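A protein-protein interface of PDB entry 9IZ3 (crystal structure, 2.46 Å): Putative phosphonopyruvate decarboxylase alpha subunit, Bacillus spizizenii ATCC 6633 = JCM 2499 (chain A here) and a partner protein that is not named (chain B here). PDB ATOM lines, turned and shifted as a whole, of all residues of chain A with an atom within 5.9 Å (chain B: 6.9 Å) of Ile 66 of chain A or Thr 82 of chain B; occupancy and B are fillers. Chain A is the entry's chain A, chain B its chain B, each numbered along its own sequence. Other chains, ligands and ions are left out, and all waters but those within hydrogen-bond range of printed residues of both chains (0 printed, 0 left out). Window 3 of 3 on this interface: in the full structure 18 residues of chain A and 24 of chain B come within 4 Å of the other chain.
The side-chain amide nitrogen of Asn 77 of chain B lies within hydrogen-bond range of the side-chain hydroxyl of Ser 70 of chain A, 3.1 Å away.
O of Pro 64 of chain A sits close to SD of Met 83 of chain B, at 3.7 Å.
SD of Met 83 of chain B is in hydrogen-bond range of N of Ile 66 of chain A (3.4 Å).
O of Arg 67 of chain A is in hydrogen-bond range of OG of Ser 65 of chain A, 2.6 Å away.
The backbone NH of Ser 65 of chain A sits at hydrogen-bond distance from the backbone carbonyl oxygen of Gly 36 of chain A, at 2.8 Å.
Among the printed residues, pairs that only touch across the chains: Ser 65 of chain A with Met 83 of chain B (3.4 Å), Ile 66 of chain A with Gly 79 of chain B (3.6 Å), Ile 66 of chain A with Thr 82 of chain B (3.5 Å) and Ser 70 of chain A with Met 83 of chain B (3.5 Å).
Of chain B, only Gly 79 (3.6 Å), Thr 82 (3.5 Å) and Met 83 (3.4 Å) come within 4 Å of Ile 66 of chain A.
Printed residues of chain A within 4 Å of Thr 82 of chain B: Ile 66 (3.5 Å).
Printed residues of chain B within 4 Å of Ser 65 of chain A: Met 83 (3.4 Å).
Of the printed residues of chain A, Met 83 of chain B touches Pro 64 (3.7 Å), Ser 65 (3.4 Å), Ile 66 (3.4 Å) and Ser 70 (3.5 Å).
Printed residues of chain A within 4 Å of Asn 77 of chain B: Ser 70 (3.1 Å).
Printed residues of chain B within 4 Å of Pro 64 of chain A: Met 83.
Gly 36 of chain A touches none of the printed residues of chain B.
The nearest printed residue of chain A that does not touch Thr 82 of chain B is Ser 65 of chain A (7.1 Å).
Of the 8 printed residues of chain A, 4 touch a printed residue of chain B.
Hydrophobic or aromatic side chains of chain A that line the printed part of chain B: Ile 66.
Among the printed residues, 7 pairs touch across the chains.
Among the printed residues, no Asp or Glu carboxylate lies within 4 Å of a Lys or Arg side-chain nitrogen of the other chain.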
ATOM      1  N   GLY A  36     -30.369  33.276  14.845  1.00  0.00           N
ATOM      2  CA  GLY A  36     -30.055  34.134  13.719  1.00  0.00           C
ATOM      3  C   GLY A  36     -28.742  33.739  13.076  1.00  0.00           C
ATOM      4  O   GLY A  36     -28.030  32.843  13.544  1.00  0.00           O
ATOM      5  N   VAL A  37     -28.440  34.426  11.984  1.00  0.00           N
ATOM      6  CA  VAL A  37     -27.182  34.263  11.258  1.00  0.00           C
ATOM      7  C   VAL A  37     -26.312  35.483  11.531  1.00  0.00           C
ATOM      8  O   VAL A  37     -26.793  36.616  11.410  1.00  0.00           O
ATOM      9  CB  VAL A  37     -27.403  34.064   9.741  1.00  0.00           C
ATOM     10  CG1 VAL A  37     -28.337  32.891   9.497  1.00  0.00           C
ATOM     11  CG2 VAL A  37     -27.963  35.315   9.074  1.00  0.00           C
ATOM     12  N   PRO A  64     -26.396  30.392  17.073  1.00  0.00           N
ATOM     13  CA  PRO A  64     -25.962  30.803  15.730  1.00  0.00           C
ATOM     14  C   PRO A  64     -26.441  29.799  14.694  1.00  0.00           C
ATOM     15  O   PRO A  64     -26.405  28.586  14.918  1.00  0.00           O
ATOM     16  CB  PRO A  64     -24.432  30.819  15.832  1.00  0.00           C
ATOM     17  CG  PRO A  64     -24.125  30.786  17.303  1.00  0.00           C
ATOM     18  CD  PRO A  64     -25.261  30.054  17.947  1.00  0.00           C
ATOM     19  N   SER A  65     -26.897  30.313  13.556  1.00  0.00           N
ATOM     20  CA  SER A  65     -27.493  29.482  12.522  1.00  0.00           C
ATOM     21  C   SER A  65     -26.787  29.686  11.188  1.00  0.00           C
ATOM     22  O   SER A  65     -26.337  30.787  10.865  1.00  0.00           O
ATOM     23  CB  SER A  65     -28.987  29.779  12.370  1.00  0.00           C
ATOM     24  OG  SER A  65     -29.520  29.103  11.245  1.00  0.00           O
ATOM     25  N   ILE A  66     -26.709  28.603  10.409  1.00  0.00           N
ATOM     26  CA  ILE A  66     -26.058  28.662   9.102  1.00  0.00           C
ATOM     27  C   ILE A  66     -26.927  29.414   8.101  1.00  0.00           C
ATOM     28  O   ILE A  66     -26.416  30.128   7.230  1.00  0.00           O
ATOM     29  CB  ILE A  66     -25.726  27.242   8.603  1.00  0.00           C
ATOM     30  CG1 ILE A  66     -26.964  26.346   8.683  1.00  0.00           C
ATOM     31  CG2 ILE A  66     -24.597  26.638   9.423  1.00  0.00           C
ATOM     32  CD1 ILE A  66     -27.196  25.516   7.454  1.00  0.00           C
ATOM     33  N   ARG A  67     -28.246  29.263   8.199  1.00  0.00           N
ATOM     34  CA  ARG A  67     -29.153  29.906   7.260  1.00  0.00           C
ATOM     35  C   ARG A  67     -30.449  30.251   7.977  1.00  0.00           C
ATOM     36  O   ARG A  67     -30.762  29.701   9.035  1.00  0.00           O
ATOM     37  CB  ARG A  67     -29.429  29.017   6.041  1.00  0.00           C
ATOM     38  CG  ARG A  67     -29.837  29.800   4.805  1.00  0.00           C
ATOM     39  CD  ARG A  67     -29.739  28.962   3.549  1.00  0.00           C
ATOM     40  NE  ARG A  67     -31.033  28.421   3.149  1.00  0.00           N
ATOM     41  CZ  ARG A  67     -31.391  28.211   1.887  1.00  0.00           C
ATOM     42  NH1 ARG A  67     -30.548  28.498   0.903  1.00  0.00           N
ATOM     43  NH2 ARG A  67     -32.588  27.713   1.607  1.00  0.00           N
ATOM     44  N   GLU A  68     -31.212  31.165   7.370  1.00  0.00           N
ATOM     45  CA  GLU A  68     -32.374  31.735   8.045  1.00  0.00           C
ATOM     46  C   GLU A  68     -33.471  30.700   8.263  1.00  0.00           C
ATOM     47  O   GLU A  68     -34.134  30.710   9.307  1.00  0.00           O
ATOM     48  CB  GLU A  68     -32.913  32.923   7.251  1.00  0.00           C
ATOM     49  CG  GLU A  68     -32.057  34.173   7.344  1.00  0.00           C
ATOM     50  CD  GLU A  68     -31.003  34.233   6.253  1.00  0.00           C
ATOM     51  OE1 GLU A  68     -31.105  33.453   5.283  1.00  0.00           O
ATOM     52  OE2 GLU A  68     -30.075  35.062   6.365  1.00  0.00           O
ATOM     53  N   SER A  70     -33.126  27.530   8.799  1.00  0.00           N
ATOM     54  CA  SER A  70     -32.742  26.722   9.951  1.00  0.00           C
ATOM     55  C   SER A  70     -32.930  27.492  11.253  1.00  0.00           C
ATOM     56  O   SER A  70     -33.327  26.913  12.271  1.00  0.00           O
ATOM     57  CB  SER A  70     -31.299  26.253   9.801  1.00  0.00           C
ATOM     58  OG  SER A  70     -31.241  25.074   9.023  1.00  0.00           O
ATOM     59  N   ASN B  77     -31.629  19.952   3.531  1.00  0.00           N
ATOM     60  CA  ASN B  77     -31.107  20.883   4.528  1.00  0.00           C
ATOM     61  C   ASN B  77     -29.958  20.216   5.284  1.00  0.00           C
ATOM     62  O   ASN B  77     -29.999  20.051   6.498  1.00  0.00           O
ATOM     63  CB  ASN B  77     -32.220  21.337   5.480  1.00  0.00           C
ATOM     64  CG  ASN B  77     -31.780  22.455   6.414  1.00  0.00           C
ATOM     65  OD1 ASN B  77     -30.844  23.201   6.117  1.00  0.00           O
ATOM     66  ND2 ASN B  77     -32.461  22.579   7.551  1.00  0.00           N
ATOM     67  N   MET B  78     -28.911  19.829   4.551  1.00  0.00           N
ATOM     68  CA  MET B  78     -27.830  19.068   5.173  1.00  0.00           C
ATOM     69  C   MET B  78     -27.064  19.900   6.194  1.00  0.00           C
ATOM     70  O   MET B  78     -26.619  19.366   7.221  1.00  0.00           O
ATOM     71  CB  MET B  78     -26.878  18.527   4.105  1.00  0.00           C
ATOM     72  CG  MET B  78     -26.074  17.321   4.568  1.00  0.00           C
ATOM     73  SD  MET B  78     -24.888  16.726   3.347  1.00  0.00           S
ATOM     74  CE  MET B  78     -23.906  18.194   3.083  1.00  0.00           C
ATOM     75  N   GLY B  79     -26.925  21.200   5.947  1.00  0.00           N
ATOM     76  CA  GLY B  79     -26.193  22.090   6.829  1.00  0.00           C
ATOM     77  C   GLY B  79     -26.604  22.033   8.285  1.00  0.00           C
ATOM     78  O   GLY B  79     -25.797  22.345   9.169  1.00  0.00           O
ATOM     79  N   ILE B  80     -27.850  21.618   8.551  1.00  0.00           N
ATOM     80  CA  ILE B  80     -28.332  21.514   9.926  1.00  0.00           C
ATOM     81  C   ILE B  80     -27.380  20.688  10.775  1.00  0.00           C
ATOM     82  O   ILE B  80     -27.169  20.990  11.959  1.00  0.00           O
ATOM     83  CB  ILE B  80     -29.766  20.936   9.963  1.00  0.00           C
ATOM     84  CG1 ILE B  80     -30.295  20.921  11.392  1.00  0.00           C
ATOM     85  CG2 ILE B  80     -29.786  19.502   9.464  1.00  0.00           C
ATOM     86  CD1 ILE B  80     -30.794  22.235  11.861  1.00  0.00           C
ATOM     87  N   ILE B  81     -26.757  19.661  10.188  1.00  0.00           N
ATOM     88  CA  ILE B  81     -25.910  18.780  10.986  1.00  0.00           C
ATOM     89  C   ILE B  81     -24.775  19.568  11.629  1.00  0.00           C
ATOM     90  O   ILE B  81     -24.398  19.310  12.780  1.00  0.00           O
ATOM     91  CB  ILE B  81     -25.393  17.602  10.135  1.00  0.00           C
ATOM     92  CG1 ILE B  81     -24.425  18.074   9.049  1.00  0.00           C
ATOM     93  CG2 ILE B  81     -26.557  16.849   9.516  1.00  0.00           C
ATOM     94  CD1 ILE B  81     -23.822  16.939   8.259  1.00  0.00           C
ATOM     95  N   THR B  82     -24.260  20.587  10.930  1.00  0.00           N
ATOM     96  CA  THR B  82     -23.178  21.389  11.493  1.00  0.00           C
ATOM     97  C   THR B  82     -23.592  22.011  12.817  1.00  0.00           C
ATOM     98  O   THR B  82     -22.808  22.045  13.771  1.00  0.00           O
ATOM     99  CB  THR B  82     -22.763  22.480  10.511  1.00  0.00           C
ATOM    100  OG1 THR B  82     -23.924  23.233  10.133  1.00  0.00           O
ATOM    101  CG2 THR B  82     -22.115  21.862   9.274  1.00  0.00           C
ATOM    102  N   MET B  83     -24.827  22.502  12.898  1.00  0.00           N
ATOM    103  CA  MET B  83     -25.301  23.041  14.163  1.00  0.00           C
ATOM    104  C   MET B  83     -25.552  21.926  15.165  1.00  0.00           C
ATOM    105  O   MET B  83     -25.162  22.038  16.337  1.00  0.00           O
ATOM    106  CB  MET B  83     -26.548  23.883  13.918  1.00  0.00           C
ATOM    107  CG  MET B  83     -26.256  24.997  12.934  1.00  0.00           C
ATOM    108  SD  MET B  83     -27.630  26.063  12.528  1.00  0.00           S
ATOM    109  CE  MET B  83     -28.774  24.911  11.823  1.00  0.00           C
ATOM    110  N   ILE B  84     -26.146  20.816  14.714  1.00  0.00           N
ATOM    111  CA  ILE B  84     -26.400  19.714  15.637  1.00  0.00           C
ATOM    112  C   ILE B  84     -25.090  19.221  16.223  1.00  0.00           C
ATOM    113  O   ILE B  84     -24.972  19.008  17.436  1.00  0.00           O
ATOM    114  CB  ILE B  84     -27.161  18.577  14.932  1.00  0.00           C
ATOM    115  CG1 ILE B  84     -28.524  19.050  14.437  1.00  0.00           C
ATOM    116  CG2 ILE B  84     -27.328  17.394  15.864  1.00  0.00           C
ATOM    117  CD1 ILE B  84     -29.287  17.942  13.745  1.00  0.00           C
ATOM    118  N   GLY B  85     -24.077  19.059  15.369  1.00  0.00           N
ATOM    119  CA  GLY B  85     -22.768  18.628  15.817  1.00  0.00           C
ATOM    120  C   GLY B  85     -22.024  19.669  16.623  1.00  0.00           C
ATOM    121  O   GLY B  85     -21.123  19.311  17.388  1.00  0.00           O
ATOM    122  N   HIS B  86     -22.380  20.950  16.477  1.00  0.00           N
ATOM    123  CA  HIS B  86     -21.754  21.964  17.321  1.00  0.00           C
ATOM    124  C   HIS B  86     -22.449  22.084  18.672  1.00  0.00           C
ATOM    125  O   HIS B  86     -21.780  22.128  19.710  1.00  0.00           O
ATOM    126  CB  HIS B  86     -21.742  23.325  16.620  1.00  0.00           C
ATOM    127  CG  HIS B  86     -21.007  24.387  17.379  1.00  0.00           C
ATOM    128  ND1 HIS B  86     -21.567  25.609  17.685  1.00  0.00           N
ATOM    129  CD2 HIS B  86     -19.758  24.402  17.903  1.00  0.00           C
ATOM    130  CE1 HIS B  86     -20.692  26.334  18.358  1.00  0.00           C
ATOM    131  NE2 HIS B  86     -19.586  25.626  18.503  1.00  0.00           N
ATOM    132  N   GLN B  87     -23.783  22.128  18.675  1.00  0.00           N
ATOM    133  CA  GLN B  87     -24.524  22.220  19.930  1.00  0.00           C
ATOM    134  C   GLN B  87     -24.383  20.953  20.764  1.00  0.00           C
ATOM    135  O   GLN B  87     -24.401  21.019  21.997  1.00  0.00           O
ATOM    136  CB  GLN B  87     -25.994  22.504  19.637  1.00  0.00           C
ATOM    137  CG  GLN B  87     -26.249  23.895  19.067  1.00  0.00           C
ATOM    138  CD  GLN B  87     -26.147  24.973  20.126  1.00  0.00           C
ATOM    139  OE1 GLN B  87     -26.794  24.895  21.172  1.00  0.00           O
ATOM    140  NE2 GLN B  87     -25.328  25.984  19.864  1.00  0.00           N
ATOM    141  N   LYS B  88     -24.230  19.803  20.113  1.00  0.00           N
ATOM    142  CA  LYS B  88     -24.091  18.514  20.770  1.00  0.00           C
ATOM    143  C   LYS B  88     -25.170  18.225  21.807  1.00  0.00           C
ATOM    144  O   LYS B  88     -24.874  18.026  22.996  1.00  0.00           O
ATOM    145  CB  LYS B  88     -22.698  18.398  21.405  1.00  0.00           C
ATOM    146  CG  LYS B  88     -21.570  18.367  20.394  1.00  0.00           C
ATOM    147  CD  LYS B  88     -20.308  17.744  20.963  1.00  0.00           C
ATOM    148  CE  LYS B  88     -19.251  17.588  19.875  1.00  0.00           C
ATOM    149  NZ  LYS B  88     -18.934  18.889  19.221  1.00  0.00           N
ATOM    150  N   VAL B 123     -18.787  16.110  11.608  1.00  0.00           N
ATOM    151  CA  VAL B 123     -19.286  17.397  12.095  1.00  0.00           C
ATOM    152  C   VAL B 123     -19.524  17.426  13.596  1.00  0.00           C
ATOM    153  O   VAL B 123     -19.986  18.450  14.116  1.00  0.00           O
ATOM    154  CB  VAL B 123     -20.594  17.798  11.390  1.00  0.00           C
ATOM    155  CG1 VAL B 123     -20.379  17.853   9.883  1.00  0.00           C
ATOM    156  CG2 VAL B 123     -21.704  16.826  11.760  1.00  0.00           C
ATOM    157  N   GLY B 124     -19.237  16.345  14.311  1.00  0.00           N
ATOM    158  CA  GLY B 124     -19.286  16.355  15.758  1.00  0.00           C
ATOM    159  C   GLY B 124     -20.317  15.460  16.417  1.00  0.00           C
ATOM    160  O   GLY B 124     -20.487  15.550  17.638  1.00  0.00           O
ATOM    161  N   TYR B 125     -21.016  14.612  15.667  1.00  0.00           N
ATOM    162  CA  TYR B 125     -21.946  13.689  16.298  1.00  0.00           C
ATOM    163  C   TYR B 125     -21.184  12.729  17.195  1.00  0.00           C
ATOM    164  O   TYR B 125     -20.031  12.382  16.933  1.00  0.00           O
ATOM    165  CB  TYR B 125     -22.738  12.893  15.262  1.00  0.00           C
ATOM    166  CG  TYR B 125     -23.932  13.607  14.675  1.00  0.00           C
ATOM    167  CD1 TYR B 125     -23.807  14.872  14.117  1.00  0.00           C
ATOM    168  CD2 TYR B 125     -25.181  12.999  14.650  1.00  0.00           C
ATOM    169  CE1 TYR B 125     -24.899  15.520  13.560  1.00  0.00           C
ATOM    170  CE2 TYR B 125     -26.276  13.638  14.097  1.00  0.00           C
ATOM    171  CZ  TYR B 125     -26.131  14.896  13.552  1.00  0.00           C
ATOM    172  OH  TYR B 125     -27.221  15.535  12.999  1.00  0.00           O
